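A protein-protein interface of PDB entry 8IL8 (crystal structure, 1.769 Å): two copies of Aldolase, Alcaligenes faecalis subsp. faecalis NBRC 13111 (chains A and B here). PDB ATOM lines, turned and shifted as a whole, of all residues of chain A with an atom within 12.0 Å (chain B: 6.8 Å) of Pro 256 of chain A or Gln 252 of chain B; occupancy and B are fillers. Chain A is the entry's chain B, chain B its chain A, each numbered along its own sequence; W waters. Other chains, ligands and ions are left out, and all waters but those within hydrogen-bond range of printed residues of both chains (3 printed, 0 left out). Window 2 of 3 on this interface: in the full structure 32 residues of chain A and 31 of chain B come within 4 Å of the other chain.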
ATOM      1  N   ARG A 249     -15.723  12.834 -15.818  1.00  0.00           N
ATOM      2  CA  ARG A 249     -15.079  11.560 -15.490  1.00  0.00           C
ATOM      3  C   ARG A 249     -15.970  10.717 -14.603  1.00  0.00           C
ATOM      4  O   ARG A 249     -16.090   9.523 -14.843  1.00  0.00           O
ATOM      5  CB  ARG A 249     -13.711  11.773 -14.825  1.00  0.00           C
ATOM      6  CG  ARG A 249     -12.731  12.491 -15.746  1.00  0.00           C
ATOM      7  CD  ARG A 249     -11.302  12.438 -15.251  1.00  0.00           C
ATOM      8  NE  ARG A 249     -11.142  13.062 -13.936  1.00  0.00           N
ATOM      9  CZ  ARG A 249     -10.875  14.351 -13.743  1.00  0.00           C
ATOM     10  NH1 ARG A 249     -10.756  15.173 -14.778  1.00  0.00           N
ATOM     11  NH2 ARG A 249     -10.758  14.833 -12.516  1.00  0.00           N
ATOM     12  N   GLN A 250     -16.620  11.326 -13.598  1.00  0.00           N
ATOM     13  CA  GLN A 250     -17.521  10.608 -12.680  1.00  0.00           C
ATOM     14  C   GLN A 250     -18.651   9.891 -13.454  1.00  0.00           C
ATOM     15  O   GLN A 250     -19.005   8.774 -13.104  1.00  0.00           O
ATOM     16  CB  GLN A 250     -18.203  11.583 -11.704  1.00  0.00           C
ATOM     17  CG  GLN A 250     -17.354  12.215 -10.624  1.00  0.00           C
ATOM     18  CD  GLN A 250     -18.286  12.921  -9.662  1.00  0.00           C
ATOM     19  OE1 GLN A 250     -18.935  13.916 -10.001  1.00  0.00           O
ATOM     20  NE2 GLN A 250     -18.424  12.404  -8.464  1.00  0.00           N
ATOM     21  N   GLN A 252     -18.635   8.591 -16.343  1.00  0.00           N
ATOM     22  CA  GLN A 252     -18.113   7.429 -17.057  1.00  0.00           C
ATOM     23  C   GLN A 252     -17.859   6.202 -16.179  1.00  0.00           C
ATOM     24  O   GLN A 252     -17.606   5.125 -16.710  1.00  0.00           O
ATOM     25  CB  GLN A 252     -16.854   7.796 -17.841  1.00  0.00           C
ATOM     26  CG  GLN A 252     -17.073   8.990 -18.727  1.00  0.00           C
ATOM     27  CD  GLN A 252     -15.856   9.306 -19.525  1.00  0.00           C
ATOM     28  OE1 GLN A 252     -15.485   8.564 -20.420  1.00  0.00           O
ATOM     29  NE2 GLN A 252     -15.224  10.440 -19.266  1.00  0.00           N
ATOM     30  N   GLY A 253     -17.934   6.359 -14.866  1.00  0.00           N
ATOM     31  CA  GLY A 253     -17.715   5.266 -13.944  1.00  0.00           C
ATOM     32  C   GLY A 253     -16.265   5.165 -13.532  1.00  0.00           C
ATOM     33  O   GLY A 253     -15.359   5.265 -14.367  1.00  0.00           O
ATOM     34  N   ILE A 254     -16.037   4.987 -12.243  1.00  0.00           N
ATOM     35  CA  ILE A 254     -14.700   4.832 -11.726  1.00  0.00           C
ATOM     36  C   ILE A 254     -14.583   3.442 -11.147  1.00  0.00           C
ATOM     37  O   ILE A 254     -15.443   3.022 -10.364  1.00  0.00           O
ATOM     38  CB  ILE A 254     -14.377   5.948 -10.709  1.00  0.00           C
ATOM     39  CG1 ILE A 254     -14.409   7.318 -11.413  1.00  0.00           C
ATOM     40  CG2 ILE A 254     -13.024   5.710 -10.044  1.00  0.00           C
ATOM     41  CD1 ILE A 254     -14.858   8.449 -10.512  1.00  0.00           C
ATOM     42  N   ALA A 255     -13.538   2.708 -11.554  1.00  0.00           N
ATOM     43  CA  ALA A 255     -13.307   1.373 -11.059  1.00  0.00           C
ATOM     44  C   ALA A 255     -12.973   1.416  -9.569  1.00  0.00           C
ATOM     45  O   ALA A 255     -12.212   2.287  -9.137  1.00  0.00           O
ATOM     46  CB  ALA A 255     -12.144   0.755 -11.811  1.00  0.00           C
ATOM     47  N   PRO A 256     -13.500   0.482  -8.767  1.00  0.00           N
ATOM     48  CA  PRO A 256     -13.091   0.434  -7.348  1.00  0.00           C
ATOM     49  C   PRO A 256     -11.601   0.108  -7.199  1.00  0.00           C
ATOM     50  O   PRO A 256     -10.984  -0.402  -8.133  1.00  0.00           O
ATOM     51  CB  PRO A 256     -13.944  -0.700  -6.768  1.00  0.00           C
ATOM     52  CG  PRO A 256     -14.264  -1.543  -7.923  1.00  0.00           C
ATOM     53  CD  PRO A 256     -14.394  -0.639  -9.111  1.00  0.00           C
ATOM     54  N   LEU A 257     -11.018   0.398  -6.036  1.00  0.00           N
ATOM     55  CA  LEU A 257      -9.623   0.076  -5.771  1.00  0.00           C
ATOM     56  C   LEU A 257      -9.476  -1.443  -5.639  1.00  0.00           C
ATOM     57  O   LEU A 257     -10.390  -2.125  -5.174  1.00  0.00           O
ATOM     58  CB  LEU A 257      -9.178   0.724  -4.446  1.00  0.00           C
ATOM     59  CG  LEU A 257      -9.083   2.247  -4.405  1.00  0.00           C
ATOM     60  CD1 LEU A 257      -8.708   2.710  -3.028  1.00  0.00           C
ATOM     61  CD2 LEU A 257      -8.117   2.773  -5.447  1.00  0.00           C
ATOM     62  N   THR A 258      -8.316  -1.969  -6.016  1.00  0.00           N
ATOM     63  CA  THR A 258      -8.030  -3.390  -5.874  1.00  0.00           C
ATOM     64  C   THR A 258      -7.422  -3.621  -4.498  1.00  0.00           C
ATOM     65  O   THR A 258      -6.547  -2.855  -4.066  1.00  0.00           O
ATOM     66  CB  THR A 258      -7.051  -3.815  -6.951  1.00  0.00           C
ATOM     67  OG1 THR A 258      -5.812  -3.125  -6.728  1.00  0.00           O
ATOM     68  CG2 THR A 258      -7.564  -3.537  -8.335  1.00  0.00           C
ATOM     69  N   PHE B  36      -8.017   4.772   0.035  1.00  0.00           N
ATOM     70  CA  PHE B  36      -9.207   4.166   0.588  1.00  0.00           C
ATOM     71  C   PHE B  36     -10.043   5.184   1.324  1.00  0.00           C
ATOM     72  O   PHE B  36     -11.254   5.193   1.138  1.00  0.00           O
ATOM     73  CB  PHE B  36      -8.877   2.958   1.471  1.00  0.00           C
ATOM     74  CG  PHE B  36      -8.759   1.707   0.643  1.00  0.00           C
ATOM     75  CD1 PHE B  36      -9.885   1.095   0.115  1.00  0.00           C
ATOM     76  CD2 PHE B  36      -7.521   1.151   0.372  1.00  0.00           C
ATOM     77  CE1 PHE B  36      -9.774  -0.067  -0.649  1.00  0.00           C
ATOM     78  CE2 PHE B  36      -7.415  -0.013  -0.392  1.00  0.00           C
ATOM     79  CZ  PHE B  36      -8.538  -0.616  -0.888  1.00  0.00           C
ATOM     80  N   ARG B  39     -12.072   7.104  -1.149  1.00  0.00           N
ATOM     81  CA  ARG B  39     -13.191   6.296  -1.638  1.00  0.00           C
ATOM     82  C   ARG B  39     -14.282   6.146  -0.582  1.00  0.00           C
ATOM     83  O   ARG B  39     -15.431   6.068  -0.941  1.00  0.00           O
ATOM     84  CB  ARG B  39     -12.738   4.916  -2.163  1.00  0.00           C
ATOM     85  CG  ARG B  39     -11.645   4.956  -3.227  1.00  0.00           C
ATOM     86  CD  ARG B  39     -12.014   5.811  -4.422  1.00  0.00           C
ATOM     87  NE  ARG B  39     -11.014   5.734  -5.488  1.00  0.00           N
ATOM     88  CZ  ARG B  39     -11.107   4.932  -6.549  1.00  0.00           C
ATOM     89  NH1 ARG B  39     -12.151   4.115  -6.689  1.00  0.00           N
ATOM     90  NH2 ARG B  39     -10.146   4.919  -7.461  1.00  0.00           N
ATOM     91  N   MET B  43     -18.090   7.407  -1.004  1.00  0.00           N
ATOM     92  CA  MET B  43     -19.166   6.453  -0.825  1.00  0.00           C
ATOM     93  C   MET B  43     -20.220   7.002   0.133  1.00  0.00           C
ATOM     94  O   MET B  43     -21.419   6.770  -0.056  1.00  0.00           O
ATOM     95  CB  MET B  43     -18.585   5.134  -0.296  1.00  0.00           C
ATOM     96  CG  MET B  43     -19.624   4.079   0.017  1.00  0.00           C
ATOM     97  SD  MET B  43     -18.848   2.558   0.615  1.00  0.00           S
ATOM     98  CE  MET B  43     -18.198   3.120   2.172  1.00  0.00           C
ATOM     99  N   ASP B 245     -11.383  -0.405   7.956  1.00  0.00           N
ATOM    100  CA  ASP B 245     -11.153  -1.552   7.087  1.00  0.00           C
ATOM    101  C   ASP B 245     -12.486  -2.078   6.521  1.00  0.00           C
ATOM    102  O   ASP B 245     -12.565  -2.399   5.333  1.00  0.00           O
ATOM    103  CB  ASP B 245     -10.361  -2.637   7.819  1.00  0.00           C
ATOM    104  CG  ASP B 245      -8.909  -2.249   8.074  1.00  0.00           C
ATOM    105  OD1 ASP B 245      -8.407  -1.336   7.390  1.00  0.00           O
ATOM    106  OD2 ASP B 245      -8.271  -2.875   8.933  1.00  0.00           O
ATOM    107  N   TRP B 247     -15.303  -0.202   5.937  1.00  0.00           N
ATOM    108  CA  TRP B 247     -15.702   0.777   4.915  1.00  0.00           C
ATOM    109  C   TRP B 247     -14.855   0.610   3.657  1.00  0.00           C
ATOM    110  O   TRP B 247     -15.379   0.713   2.564  1.00  0.00           O
ATOM    111  CB  TRP B 247     -15.540   2.196   5.476  1.00  0.00           C
ATOM    112  CG  TRP B 247     -16.502   2.559   6.571  1.00  0.00           C
ATOM    113  CD1 TRP B 247     -17.770   2.078   6.753  1.00  0.00           C
ATOM    114  CD2 TRP B 247     -16.308   3.571   7.568  1.00  0.00           C
ATOM    115  NE1 TRP B 247     -18.372   2.728   7.804  1.00  0.00           N
ATOM    116  CE2 TRP B 247     -17.494   3.643   8.329  1.00  0.00           C
ATOM    117  CE3 TRP B 247     -15.236   4.419   7.898  1.00  0.00           C
ATOM    118  CZ2 TRP B 247     -17.642   4.535   9.391  1.00  0.00           C
ATOM    119  CZ3 TRP B 247     -15.376   5.285   8.968  1.00  0.00           C
ATOM    120  CH2 TRP B 247     -16.568   5.333   9.704  1.00  0.00           C
ATOM    121  N   SER B 248     -13.556   0.302   3.812  1.00  0.00           N
ATOM    122  CA  SER B 248     -12.652   0.050   2.686  1.00  0.00           C
ATOM    123  C   SER B 248     -13.162  -1.137   1.857  1.00  0.00           C
ATOM    124  O   SER B 248     -13.261  -1.031   0.634  1.00  0.00           O
ATOM    125  CB  SER B 248     -11.235  -0.223   3.184  1.00  0.00           C
ATOM    126  OG  SER B 248     -10.694   0.928   3.813  1.00  0.00           O
ATOM    127  N   ARG B 249     -13.546  -2.245   2.524  1.00  0.00           N
ATOM    128  CA  ARG B 249     -14.101  -3.408   1.824  1.00  0.00           C
ATOM    129  C   ARG B 249     -15.368  -3.048   1.090  1.00  0.00           C
ATOM    130  O   ARG B 249     -15.527  -3.442  -0.060  1.00  0.00           O
ATOM    131  CB  ARG B 249     -14.343  -4.577   2.782  1.00  0.00           C
ATOM    132  CG  ARG B 249     -13.069  -5.096   3.411  1.00  0.00           C
ATOM    133  CD  ARG B 249     -13.255  -6.438   4.099  1.00  0.00           C
ATOM    134  NE  ARG B 249     -14.245  -6.402   5.176  1.00  0.00           N
ATOM    135  CZ  ARG B 249     -13.980  -6.091   6.439  1.00  0.00           C
ATOM    136  NH1 ARG B 249     -12.741  -5.764   6.807  1.00  0.00           N
ATOM    137  NH2 ARG B 249     -14.952  -6.083   7.343  1.00  0.00           N
ATOM    138  N   GLN B 250     -16.256  -2.261   1.719  1.00  0.00           N
ATOM    139  CA  GLN B 250     -17.502  -1.813   1.086  1.00  0.00           C
ATOM    140  C   GLN B 250     -17.238  -1.066  -0.247  1.00  0.00           C
ATOM    141  O   GLN B 250     -17.964  -1.283  -1.207  1.00  0.00           O
ATOM    142  CB  GLN B 250     -18.248  -0.826   1.997  1.00  0.00           C
ATOM    143  CG  GLN B 250     -18.899  -1.380   3.233  1.00  0.00           C
ATOM    144  CD  GLN B 250     -19.772  -0.292   3.827  1.00  0.00           C
ATOM    145  OE1 GLN B 250     -19.285   0.741   4.307  1.00  0.00           O
ATOM    146  NE2 GLN B 250     -21.071  -0.467   3.758  1.00  0.00           N
ATOM    147  N   THR B 251     -16.227  -0.162  -0.283  1.00  0.00           N
ATOM    148  CA  THR B 251     -15.943   0.600  -1.493  1.00  0.00           C
ATOM    149  C   THR B 251     -15.559  -0.310  -2.670  1.00  0.00           C
ATOM    150  O   THR B 251     -15.815   0.038  -3.824  1.00  0.00           O
ATOM    151  CB  THR B 251     -14.855   1.671  -1.271  1.00  0.00           C
ATOM    152  OG1 THR B 251     -13.593   1.040  -1.147  1.00  0.00           O
ATOM    153  CG2 THR B 251     -15.134   2.588  -0.113  1.00  0.00           C
ATOM    154  N   GLN B 252     -14.927  -1.452  -2.387  1.00  0.00           N
ATOM    155  CA  GLN B 252     -14.500  -2.376  -3.431  1.00  0.00           C
ATOM    156  C   GLN B 252     -15.619  -3.190  -4.067  1.00  0.00           C
ATOM    157  O   GLN B 252     -15.397  -3.808  -5.106  1.00  0.00           O
ATOM    158  CB  GLN B 252     -13.409  -3.303  -2.914  1.00  0.00           C
ATOM    159  CG  GLN B 252     -12.271  -2.545  -2.296  1.00  0.00           C
ATOM    160  CD  GLN B 252     -11.195  -3.458  -1.825  1.00  0.00           C
ATOM    161  OE1 GLN B 252     -11.382  -4.277  -0.933  1.00  0.00           O
ATOM    162  NE2 GLN B 252     -10.034  -3.318  -2.405  1.00  0.00           N
ATOM    163  N   GLY B 253     -16.804  -3.177  -3.475  1.00  0.00           N
ATOM    164  CA  GLY B 253     -17.931  -3.910  -4.011  1.00  0.00           C
ATOM    165  C   GLY B 253     -18.024  -5.289  -3.400  1.00  0.00           C
ATOM    166  O   GLY B 253     -17.017  -5.986  -3.247  1.00  0.00           O
ATOM    167  N   ILE B 254     -19.224  -5.674  -3.025  1.00  0.00           N
ATOM    168  CA  ILE B 254     -19.462  -6.979  -2.439  1.00  0.00           C
ATOM    169  C   ILE B 254     -20.368  -7.737  -3.355  1.00  0.00           C
ATOM    170  O   ILE B 254     -21.398  -7.209  -3.767  1.00  0.00           O
ATOM    171  CB  ILE B 254     -20.022  -6.849  -1.003  1.00  0.00           C
ATOM    172  CG1 ILE B 254     -18.994  -6.130  -0.094  1.00  0.00           C
ATOM    173  CG2 ILE B 254     -20.429  -8.223  -0.439  1.00  0.00           C
ATOM    174  CD1 ILE B 254     -19.635  -5.246   0.949  1.00  0.00           C
HETATM  175  O   HOH W   1     -12.076  -4.150  -6.041  1.00  0.00           O
HETATM  176  O   HOH W   2      -9.876   3.133  -9.603  1.00  0.00           O
HETATM  177  O   HOH W   3     -12.670   1.394  -3.932  1.00  0.00           O
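NH1 of Arg 39 of chain B is in hydrogen-bond range of O of Ala 255 of chain A, at 3.1 Å.
The backbone carbonyl oxygen (O) of Leu 257 of chain A lies within hydrogen-bond range of the side-chain amide nitrogen (NE2) of Gln 252 of chain B (3.0 Å).
The backbone carbonyl oxygen (O) of Ser 248 of chain B is in hydrogen-bond range of the side-chain hydroxyl (OG1) of Thr 251 of chain B (2.8 Å).
Ile 254 of chain A touches Arg 39 of chain B.
Arg 39 of chain B touches Pro 256 of chain A (NH1 to CA, 3.9 Å).
CB of Pro 256 of chain A touches O of Thr 251 of chain B (3.6 Å).
Pro 256 of chain A touches Gln 252 of chain B.
Leu 257 of chain A touches Phe 36 of chain B.
Leu 257 of chain A touches Arg 39 of chain B.
Gln 252 of chain B touches Thr 258 of chain A.
Pro 256 of chain A touches three residues of chain B.
Of the printed residues of chain B, Leu 257 of chain A touches Phe 36, Arg 39 and Gln 252.
Of the printed residues of chain A, Arg 39 of chain B touches Ile 254 (3.8 Å), Ala 255 (3.1 Å), Pro 256 (3.9 Å) and Leu 257 (3.6 Å).
Trp 247 of chain B touches none of the printed residues of chain A.
No residue of chain A comes within 4 Å of Ser 248 of chain B.
Gln 252 of chain B touches just these residues of chain A: Pro 256, Leu 257 and Thr 258.
No residue of chain A comes within 4 Å of Gly 253 of chain B.
No residue of chain A comes within 4 Å of Ile 254 of chain B.
The nearest residue of chain B that does not touch Pro 256 of chain A is Gly 253 of chain B (5.0 Å).
Hydrophobic or aromatic side chains of chain A that line the printed part of chain B: Ile 254, Pro 256 and Leu 257.
Positions printed for both chains: 249, 250, 252, 253 and 254.
Water W2 lies within hydrogen-bond range of the backbone carbonyl oxygen of Ala 255 of chain A (2.5 Å) and the guanidinium group of Arg 39 of chain B (2.8 Å).
Water W1 bridges the backbone carbonyl oxygen (O) of Leu 257 of chain A and the backbone carbonyl oxygen (O) of Gln 252 of chain B.
Water W3 bridges the backbone NH (N) of Leu 257 of chain A and the side-chain hydroxyl (OG1) of Thr 251 of chain B.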
